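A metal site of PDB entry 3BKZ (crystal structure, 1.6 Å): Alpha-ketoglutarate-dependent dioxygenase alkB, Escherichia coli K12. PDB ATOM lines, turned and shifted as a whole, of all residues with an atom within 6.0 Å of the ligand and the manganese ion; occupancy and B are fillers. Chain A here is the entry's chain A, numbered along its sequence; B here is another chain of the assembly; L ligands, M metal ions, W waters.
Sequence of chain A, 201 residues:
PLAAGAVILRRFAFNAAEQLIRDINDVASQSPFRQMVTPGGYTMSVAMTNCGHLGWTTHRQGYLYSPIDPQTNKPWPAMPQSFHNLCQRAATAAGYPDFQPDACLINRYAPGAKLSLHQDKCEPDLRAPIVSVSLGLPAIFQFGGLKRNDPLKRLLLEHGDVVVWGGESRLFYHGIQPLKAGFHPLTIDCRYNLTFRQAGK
CD2 of Leu 105 touches O1 of the ligand, 3.3 Å away.
CD2 of Leu 115 touches C2 of the ligand, at 3.3 Å.
OG of Ser 132 touches O5 of the ligand, 3.8 Å away.
Ile 176 touches the ligand.
Thr 195 touches the ligand (OG1 to C3, 3.7 Å).
2YR 8 of chain B touches the ligand.
Hydrophobic or aromatic side chains within 4 Å of the ligand: Leu 105, Tyr 109, Leu 115, His 118, His 174 and Ile 176.
Of the 21 residues printed, 14 come within 4 Å of the ligand.
The nearest printed residue that does not touch the ligand is Phe 141 (4.3 Å).
The side-chain hydroxyl (OH) of Tyr 109 sits at hydrogen-bond distance from an oxygen (O4) of the ligand (2.7 Å).
O2 of the ligand lies close to NH2 of Arg 197 (2.9 Å).
An oxygen (O1) of the ligand lies close to the side-chain amide oxygen of Asn 107 (2.9 Å).
The guanidinium group (NH1) of Arg 191 is in salt-bridge range of an oxygen (O4) of the ligand, 2.9 Å away.
The side-chain amide nitrogen of Asn 193 sits at hydrogen-bond distance from an oxygen (O5) of the ligand (3.3 Å).
The manganese ion is bound by a ring nitrogen (NE2) of His 118 (2.2 Å), a ring nitrogen (NE2) of His 174 (2.2 Å), the side-chain carboxylate of Asp 120 (2.2 Å), water W4 (2.3 Å), an oxygen (O2) of the ligand (2.3 Å) and an oxygen (O3) of the ligand (2.3 Å).
The manganese ion has six donor atoms within binding distance.
Water W4 bridges the side-chain carboxylate (OD2) of Asp 120 (2.4 Å) and the guanidinium group (NH2) of Arg 197 (3.3 Å).
Water W2 bridges an oxygen (O5) of the ligand and the side-chain hydroxyl (OG) of Ser 132.
Water W3 lies within hydrogen-bond range of OG1 of Thr 195 (2.7 Å) and OG of Ser 132 (2.9 Å).
Water W1 bridges N3 of 2YR 8 of chain B (2.8 Å) and NH2 of Arg 197 (3.0 Å).
OD2 of Asp 120 is in salt-bridge range of NE of Arg 197 (3.0 Å).
N of Tyr 109 sits at hydrogen-bond distance from O of Arg 191 (2.8 Å).
The side-chain hydroxyl of Ser 134 sits at hydrogen-bond distance from the guanidinium group of Arg 191, 2.8 Å away.
The side-chain amide oxygen of Asn 193 lies within hydrogen-bond range of the side-chain hydroxyl of Thr 195, 2.7 Å away.
ND2 of Asn 193 sits at hydrogen-bond distance from OG of Ser 132.
ND2 of Asn 193 lies close to O of Val 133, 3.1 Å away.
The backbone NH of Thr 195 is in hydrogen-bond range of the backbone carbonyl oxygen of Leu 105, 2.8 Å away.
N4 of 2YR 8 of chain B sits at hydrogen-bond distance from the backbone carbonyl oxygen of Gln 119, at 3.5 Å.
Merely in contact with the manganese ion: Arg 197 (3.8 Å).
Of the 21 residues printed, 4 come within 4 Å of the manganese ion.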
ATOM      1  N   LEU A 105      -7.449 -15.566   4.434  1.00  0.00           N
ATOM      2  CA  LEU A 105      -7.832 -14.195   4.765  1.00  0.00           C
ATOM      3  C   LEU A 105      -8.945 -13.742   3.814  1.00  0.00           C
ATOM      4  O   LEU A 105      -8.832 -13.902   2.603  1.00  0.00           O
ATOM      5  CB  LEU A 105      -6.622 -13.270   4.645  1.00  0.00           C
ATOM      6  CG  LEU A 105      -6.784 -11.762   4.814  1.00  0.00           C
ATOM      7  CD1 LEU A 105      -7.268 -11.420   6.207  1.00  0.00           C
ATOM      8  CD2 LEU A 105      -5.459 -11.084   4.532  1.00  0.00           C
ATOM      9  N   ASN A 107     -10.730 -10.461   2.569  1.00  0.00           N
ATOM     10  CA  ASN A 107     -10.654  -9.001   2.500  1.00  0.00           C
ATOM     11  C   ASN A 107     -11.902  -8.435   1.837  1.00  0.00           C
ATOM     12  O   ASN A 107     -12.335  -8.956   0.797  1.00  0.00           O
ATOM     13  CB  ASN A 107      -9.433  -8.557   1.689  1.00  0.00           C
ATOM     14  CG  ASN A 107      -8.122  -8.965   2.328  1.00  0.00           C
ATOM     15  OD1 ASN A 107      -7.271  -9.577   1.671  1.00  0.00           O
ATOM     16  ND2 ASN A 107      -7.951  -8.624   3.593  1.00  0.00           N
ATOM     17  N   TYR A 109     -13.316  -4.820   0.264  1.00  0.00           N
ATOM     18  CA  TYR A 109     -12.997  -3.480  -0.183  1.00  0.00           C
ATOM     19  C   TYR A 109     -14.270  -2.707  -0.498  1.00  0.00           C
ATOM     20  O   TYR A 109     -15.001  -3.064  -1.422  1.00  0.00           O
ATOM     21  CB  TYR A 109     -12.132  -3.528  -1.457  1.00  0.00           C
ATOM     22  CG  TYR A 109     -10.752  -4.114  -1.287  1.00  0.00           C
ATOM     23  CD1 TYR A 109     -10.569  -5.502  -1.192  1.00  0.00           C
ATOM     24  CD2 TYR A 109      -9.632  -3.297  -1.244  1.00  0.00           C
ATOM     25  CE1 TYR A 109      -9.288  -6.044  -1.047  1.00  0.00           C
ATOM     26  CE2 TYR A 109      -8.351  -3.830  -1.096  1.00  0.00           C
ATOM     27  CZ  TYR A 109      -8.189  -5.199  -0.998  1.00  0.00           C
ATOM     28  OH  TYR A 109      -6.928  -5.723  -0.852  1.00  0.00           O
ATOM     29  N   LEU A 115      -4.920  -1.369  -0.567  1.00  0.00           N
ATOM     30  CA  LEU A 115      -3.910  -2.084   0.187  1.00  0.00           C
ATOM     31  C   LEU A 115      -2.568  -1.633  -0.345  1.00  0.00           C
ATOM     32  O   LEU A 115      -2.204  -1.947  -1.474  1.00  0.00           O
ATOM     33  CB  LEU A 115      -4.114  -3.591   0.069  1.00  0.00           C
ATOM     34  CG  LEU A 115      -3.440  -4.488   1.110  1.00  0.00           C
ATOM     35  CD1 LEU A 115      -3.866  -4.126   2.519  1.00  0.00           C
ATOM     36  CD2 LEU A 115      -3.793  -5.905   0.803  1.00  0.00           C
ATOM     37  N   HIS A 118       3.197  -4.059  -0.233  1.00  0.00           N
ATOM     38  CA  HIS A 118       3.760  -4.852   0.853  1.00  0.00           C
ATOM     39  C   HIS A 118       4.218  -6.214   0.336  1.00  0.00           C
ATOM     40  O   HIS A 118       3.824  -6.631  -0.760  1.00  0.00           O
ATOM     41  CB  HIS A 118       2.708  -5.066   1.947  1.00  0.00           C
ATOM     42  CG  HIS A 118       1.559  -5.911   1.506  1.00  0.00           C
ATOM     43  ND1 HIS A 118       0.497  -5.406   0.773  1.00  0.00           N
ATOM     44  CD2 HIS A 118       1.303  -7.241   1.659  1.00  0.00           C
ATOM     45  CE1 HIS A 118      -0.358  -6.380   0.515  1.00  0.00           C
ATOM     46  NE2 HIS A 118       0.110  -7.500   1.033  1.00  0.00           N
ATOM     47  N   GLN A 119       5.037  -6.900   1.128  1.00  0.00           N
ATOM     48  CA  GLN A 119       5.383  -8.301   0.888  1.00  0.00           C
ATOM     49  C   GLN A 119       4.622  -9.176   1.880  1.00  0.00           C
ATOM     50  O   GLN A 119       4.408  -8.782   3.019  1.00  0.00           O
ATOM     51  CB  GLN A 119       6.878  -8.543   1.123  1.00  0.00           C
ATOM     52  CG  GLN A 119       7.808  -7.739   0.267  1.00  0.00           C
ATOM     53  CD  GLN A 119       9.256  -7.897   0.700  1.00  0.00           C
ATOM     54  OE1 GLN A 119       9.657  -7.392   1.750  1.00  0.00           O
ATOM     55  NE2 GLN A 119      10.043  -8.605  -0.105  1.00  0.00           N
ATOM     56  N   ASP A 120       4.231 -10.376   1.432  1.00  0.00           N
ATOM     57  CA  ASP A 120       3.723 -11.407   2.335  1.00  0.00           C
ATOM     58  C   ASP A 120       4.933 -12.149   2.883  1.00  0.00           C
ATOM     59  O   ASP A 120       5.464 -13.030   2.211  1.00  0.00           O
ATOM     60  CB  ASP A 120       2.815 -12.393   1.585  1.00  0.00           C
ATOM     61  CG  ASP A 120       1.445 -11.821   1.254  1.00  0.00           C
ATOM     62  OD1 ASP A 120       1.227 -10.602   1.364  1.00  0.00           O
ATOM     63  OD2 ASP A 120       0.582 -12.640   0.862  1.00  0.00           O
ATOM     64  N   SER A 132      -4.699 -16.147  -4.584  1.00  0.00           N
ATOM     65  CA  SER A 132      -5.449 -14.908  -4.350  1.00  0.00           C
ATOM     66  C   SER A 132      -6.659 -14.820  -5.294  1.00  0.00           C
ATOM     67  O   SER A 132      -6.489 -14.692  -6.510  1.00  0.00           O
ATOM     68  CB  SER A 132      -4.510 -13.713  -4.560  1.00  0.00           C
ATOM     69  OG  SER A 132      -5.083 -12.507  -4.071  1.00  0.00           O
ATOM     70  N   VAL A 133      -7.861 -14.874  -4.729  1.00  0.00           N
ATOM     71  CA  VAL A 133      -9.113 -14.905  -5.496  1.00  0.00           C
ATOM     72  C   VAL A 133      -9.857 -13.563  -5.462  1.00  0.00           C
ATOM     73  O   VAL A 133     -10.092 -13.015  -4.385  1.00  0.00           O
ATOM     74  CB  VAL A 133     -10.058 -16.027  -4.976  1.00  0.00           C
ATOM     75  CG1 VAL A 133     -11.321 -16.143  -5.846  1.00  0.00           C
ATOM     76  CG2 VAL A 133      -9.323 -17.360  -4.902  1.00  0.00           C
ATOM     77  N   SER A 134     -10.247 -13.065  -6.641  1.00  0.00           N
ATOM     78  CA  SER A 134     -11.005 -11.806  -6.753  1.00  0.00           C
ATOM     79  C   SER A 134     -12.485 -12.067  -6.984  1.00  0.00           C
ATOM     80  O   SER A 134     -12.851 -12.899  -7.812  1.00  0.00           O
ATOM     81  CB  SER A 134     -10.469 -10.961  -7.902  1.00  0.00           C
ATOM     82  OG  SER A 134      -9.171 -10.470  -7.641  1.00  0.00           O
ATOM     83  N   PHE A 141      -4.512  -4.274  -9.460  1.00  0.00           N
ATOM     84  CA  PHE A 141      -3.530  -5.012  -8.665  1.00  0.00           C
ATOM     85  C   PHE A 141      -2.126  -4.612  -9.085  1.00  0.00           C
ATOM     86  O   PHE A 141      -1.816  -4.618 -10.276  1.00  0.00           O
ATOM     87  CB  PHE A 141      -3.753  -6.506  -8.899  1.00  0.00           C
ATOM     88  CG  PHE A 141      -2.823  -7.414  -8.146  1.00  0.00           C
ATOM     89  CD1 PHE A 141      -2.854  -7.461  -6.751  1.00  0.00           C
ATOM     90  CD2 PHE A 141      -1.956  -8.271  -8.823  1.00  0.00           C
ATOM     91  CE1 PHE A 141      -2.007  -8.318  -6.050  1.00  0.00           C
ATOM     92  CE2 PHE A 141      -1.105  -9.133  -8.134  1.00  0.00           C
ATOM     93  CZ  PHE A 141      -1.137  -9.158  -6.743  1.00  0.00           C
ATOM     94  N   LEU A 157      -7.977  -6.772 -12.017  1.00  0.00           N
ATOM     95  CA  LEU A 157      -8.509  -8.050 -11.579  1.00  0.00           C
ATOM     96  C   LEU A 157     -10.016  -7.951 -11.521  1.00  0.00           C
ATOM     97  O   LEU A 157     -10.571  -7.088 -10.828  1.00  0.00           O
ATOM     98  CB  LEU A 157      -7.963  -8.451 -10.203  1.00  0.00           C
ATOM     99  CG  LEU A 157      -6.444  -8.570 -10.053  1.00  0.00           C
ATOM    100  CD1 LEU A 157      -6.085  -9.022  -8.653  1.00  0.00           C
ATOM    101  CD2 LEU A 157      -5.856  -9.526 -11.089  1.00  0.00           C
ATOM    102  N   TRP A 165       1.222 -16.618  -6.785  1.00  0.00           N
ATOM    103  CA  TRP A 165       2.661 -16.379  -6.834  1.00  0.00           C
ATOM    104  C   TRP A 165       3.412 -17.241  -5.822  1.00  0.00           C
ATOM    105  O   TRP A 165       2.863 -17.640  -4.801  1.00  0.00           O
ATOM    106  CB  TRP A 165       3.025 -14.891  -6.758  1.00  0.00           C
ATOM    107  CG  TRP A 165       2.614 -14.144  -5.511  1.00  0.00           C
ATOM    108  CD1 TRP A 165       3.412 -13.825  -4.449  1.00  0.00           C
ATOM    109  CD2 TRP A 165       1.325 -13.563  -5.230  1.00  0.00           C
ATOM    110  NE1 TRP A 165       2.702 -13.110  -3.511  1.00  0.00           N
ATOM    111  CE2 TRP A 165       1.420 -12.935  -3.963  1.00  0.00           C
ATOM    112  CE3 TRP A 165       0.099 -13.532  -5.919  1.00  0.00           C
ATOM    113  CZ2 TRP A 165       0.328 -12.276  -3.377  1.00  0.00           C
ATOM    114  CZ3 TRP A 165      -0.985 -12.876  -5.322  1.00  0.00           C
ATOM    115  CH2 TRP A 165      -0.858 -12.254  -4.062  1.00  0.00           C
ATOM    116  N   HIS A 174       3.414  -6.246  -3.648  1.00  0.00           N
ATOM    117  CA  HIS A 174       2.127  -6.188  -4.339  1.00  0.00           C
ATOM    118  C   HIS A 174       1.136  -5.345  -3.539  1.00  0.00           C
ATOM    119  O   HIS A 174       1.364  -5.057  -2.365  1.00  0.00           O
ATOM    120  CB  HIS A 174       1.563  -7.595  -4.554  1.00  0.00           C
ATOM    121  CG  HIS A 174       1.391  -8.358  -3.283  1.00  0.00           C
ATOM    122  ND1 HIS A 174       2.417  -9.047  -2.677  1.00  0.00           N
ATOM    123  CD2 HIS A 174       0.309  -8.519  -2.474  1.00  0.00           C
ATOM    124  CE1 HIS A 174       1.975  -9.604  -1.559  1.00  0.00           C
ATOM    125  NE2 HIS A 174       0.704  -9.304  -1.417  1.00  0.00           N
ATOM    126  N   GLY A 175       0.038  -4.964  -4.180  1.00  0.00           N
ATOM    127  CA  GLY A 175      -1.001  -4.195  -3.497  1.00  0.00           C
ATOM    128  C   GLY A 175      -2.217  -3.972  -4.369  1.00  0.00           C
ATOM    129  O   GLY A 175      -2.278  -4.451  -5.498  1.00  0.00           O
ATOM    130  N   ILE A 176      -3.181  -3.240  -3.822  1.00  0.00           N
ATOM    131  CA  ILE A 176      -4.431  -2.928  -4.512  1.00  0.00           C
ATOM    132  C   ILE A 176      -4.674  -1.413  -4.451  1.00  0.00           C
ATOM    133  O   ILE A 176      -4.635  -0.815  -3.373  1.00  0.00           O
ATOM    134  CB  ILE A 176      -5.643  -3.689  -3.895  1.00  0.00           C
ATOM    135  CG1 ILE A 176      -5.534  -5.203  -4.161  1.00  0.00           C
ATOM    136  CG2 ILE A 176      -6.983  -3.098  -4.386  1.00  0.00           C
ATOM    137  CD1 ILE A 176      -5.919  -5.669  -5.578  1.00  0.00           C
ATOM    138  N   ARG A 191     -15.719  -5.253  -3.346  1.00  0.00           N
ATOM    139  CA  ARG A 191     -14.864  -6.326  -3.828  1.00  0.00           C
ATOM    140  C   ARG A 191     -14.479  -7.210  -2.655  1.00  0.00           C
ATOM    141  O   ARG A 191     -14.113  -6.704  -1.579  1.00  0.00           O
ATOM    142  CB  ARG A 191     -13.602  -5.758  -4.487  1.00  0.00           C
ATOM    143  CG  ARG A 191     -12.582  -6.818  -4.871  1.00  0.00           C
ATOM    144  CD  ARG A 191     -11.360  -6.210  -5.534  1.00  0.00           C
ATOM    145  NE  ARG A 191     -10.415  -7.243  -5.956  1.00  0.00           N
ATOM    146  CZ  ARG A 191      -9.339  -7.610  -5.261  1.00  0.00           C
ATOM    147  NH1 ARG A 191      -9.059  -7.018  -4.110  1.00  0.00           N
ATOM    148  NH2 ARG A 191      -8.542  -8.560  -5.715  1.00  0.00           N
ATOM    149  N   ASN A 193     -11.777 -10.373  -1.591  1.00  0.00           N
ATOM    150  CA  ASN A 193     -10.601 -11.144  -1.963  1.00  0.00           C
ATOM    151  C   ASN A 193     -10.385 -12.270  -0.959  1.00  0.00           C
ATOM    152  O   ASN A 193     -10.567 -12.070   0.241  1.00  0.00           O
ATOM    153  CB  ASN A 193      -9.376 -10.238  -2.053  1.00  0.00           C
ATOM    154  CG  ASN A 193      -8.073 -11.010  -2.009  1.00  0.00           C
ATOM    155  OD1 ASN A 193      -7.484 -11.189  -0.939  1.00  0.00           O
ATOM    156  ND2 ASN A 193      -7.620 -11.498  -3.166  1.00  0.00           N
ATOM    157  N   THR A 195      -7.426 -14.710   0.261  1.00  0.00           N
ATOM    158  CA  THR A 195      -5.989 -14.962   0.206  1.00  0.00           C
ATOM    159  C   THR A 195      -5.644 -16.219   1.011  1.00  0.00           C
ATOM    160  O   THR A 195      -5.737 -16.219   2.238  1.00  0.00           O
ATOM    161  CB  THR A 195      -5.179 -13.736   0.695  1.00  0.00           C
ATOM    162  OG1 THR A 195      -5.373 -12.638  -0.207  1.00  0.00           O
ATOM    163  CG2 THR A 195      -3.693 -14.063   0.763  1.00  0.00           C
ATOM    164  N   ARG A 197      -3.016 -19.060   2.343  1.00  0.00           N
ATOM    165  CA  ARG A 197      -1.616 -19.211   2.706  1.00  0.00           C
ATOM    166  C   ARG A 197      -1.385 -20.481   3.529  1.00  0.00           C
ATOM    167  O   ARG A 197      -2.311 -20.979   4.174  1.00  0.00           O
ATOM    168  CB  ARG A 197      -1.107 -18.005   3.507  1.00  0.00           C
ATOM    169  CG  ARG A 197      -1.330 -16.640   2.855  1.00  0.00           C
ATOM    170  CD  ARG A 197      -0.524 -15.536   3.538  1.00  0.00           C
ATOM    171  NE  ARG A 197      -0.813 -14.222   2.974  1.00  0.00           N
ATOM    172  CZ  ARG A 197      -1.296 -13.183   3.651  1.00  0.00           C
ATOM    173  NH1 ARG A 197      -1.524 -13.268   4.955  1.00  0.00           N
ATOM    174  NH2 ARG A 197      -1.521 -12.025   3.028  1.00  0.00           N
ATOM    175  P   2YR B   8       3.723  -2.601   5.277  1.00  0.00           P
ATOM    176  OP1 2YR B   8       3.951  -3.509   6.425  1.00  0.00           O
ATOM    177  OP2 2YR B   8       4.344  -2.927   3.967  1.00  0.00           O
ATOM    178  O5' 2YR B   8       2.144  -2.419   5.115  1.00  0.00           O
ATOM    179  C5' 2YR B   8       1.535  -1.850   3.961  1.00  0.00           C
ATOM    180  C4' 2YR B   8       0.061  -2.245   3.934  1.00  0.00           C
ATOM    181  O4' 2YR B   8      -0.036  -3.669   3.670  1.00  0.00           O
ATOM    182  C3' 2YR B   8      -0.719  -2.032   5.233  1.00  0.00           C
ATOM    183  O3' 2YR B   8      -2.087  -1.730   4.965  1.00  0.00           O
ATOM    184  C2' 2YR B   8      -0.627  -3.388   5.929  1.00  0.00           C
ATOM    185  C1' 2YR B   8      -0.681  -4.330   4.740  1.00  0.00           C
ATOM    186  N1  2YR B   8       0.004  -5.646   4.917  1.00  0.00           N
ATOM    187  C2  2YR B   8      -0.709  -6.847   4.783  1.00  0.00           C
ATOM    188  O2  2YR B   8      -1.922  -6.819   4.521  1.00  0.00           O
ATOM    189  N3  2YR B   8      -0.052  -8.024   4.945  1.00  0.00           N
ATOM    190  C4  2YR B   8       1.259  -8.029   5.221  1.00  0.00           C
ATOM    191  N4  2YR B   8       1.897  -9.194   5.374  1.00  0.00           N
ATOM    192  C5  2YR B   8       2.002  -6.827   5.361  1.00  0.00           C
ATOM    193  C6  2YR B   8       1.345  -5.672   5.202  1.00  0.00           C
ATOM    194  S   2YR B   8       2.599 -10.873   7.864  1.00  0.00           S
ATOM    195  C8  2YR B   8       2.115 -11.456   6.222  1.00  0.00           C
ATOM    196  C9  2YR B   8       1.188 -10.470   5.557  1.00  0.00           C
HETATM  197  C1  LIG L   1      -3.347  -9.336   1.271  1.00  0.00           C
HETATM  198  O1  LIG L   1      -4.422  -9.333   1.919  1.00  0.00           O
HETATM  199  O2  LIG L   1      -2.249  -9.525   1.834  1.00  0.00           O
HETATM  200  C2  LIG L   1      -3.392  -9.072  -0.165  1.00  0.00           C
HETATM  201  O3  LIG L   1      -2.348  -8.891  -0.771  1.00  0.00           O
HETATM  202  C3  LIG L   1      -4.740  -9.017  -0.858  1.00  0.00           C
HETATM  203  C4  LIG L   1      -4.624  -8.531  -2.300  1.00  0.00           C
HETATM  204  C5  LIG L   1      -5.973  -8.457  -2.987  1.00  0.00           C
HETATM  205  O4  LIG L   1      -6.970  -8.026  -2.350  1.00  0.00           O
HETATM  206  O5  LIG L   1      -6.054  -8.823  -4.181  1.00  0.00           O
HETATM  207 MN    MN M   1      -0.443  -9.496   0.412  1.00  0.00          MN
HETATM  208  O   HOH W   1      -1.986  -9.970   5.198  1.00  0.00           O
HETATM  209  O   HOH W   2      -4.776 -10.458  -5.827  1.00  0.00           O
HETATM  210  O   HOH W   3      -3.371 -11.840  -1.809  1.00  0.00           O
HETATM  211  O   HOH W   4      -1.289 -11.532  -0.210  1.00  0.00           O
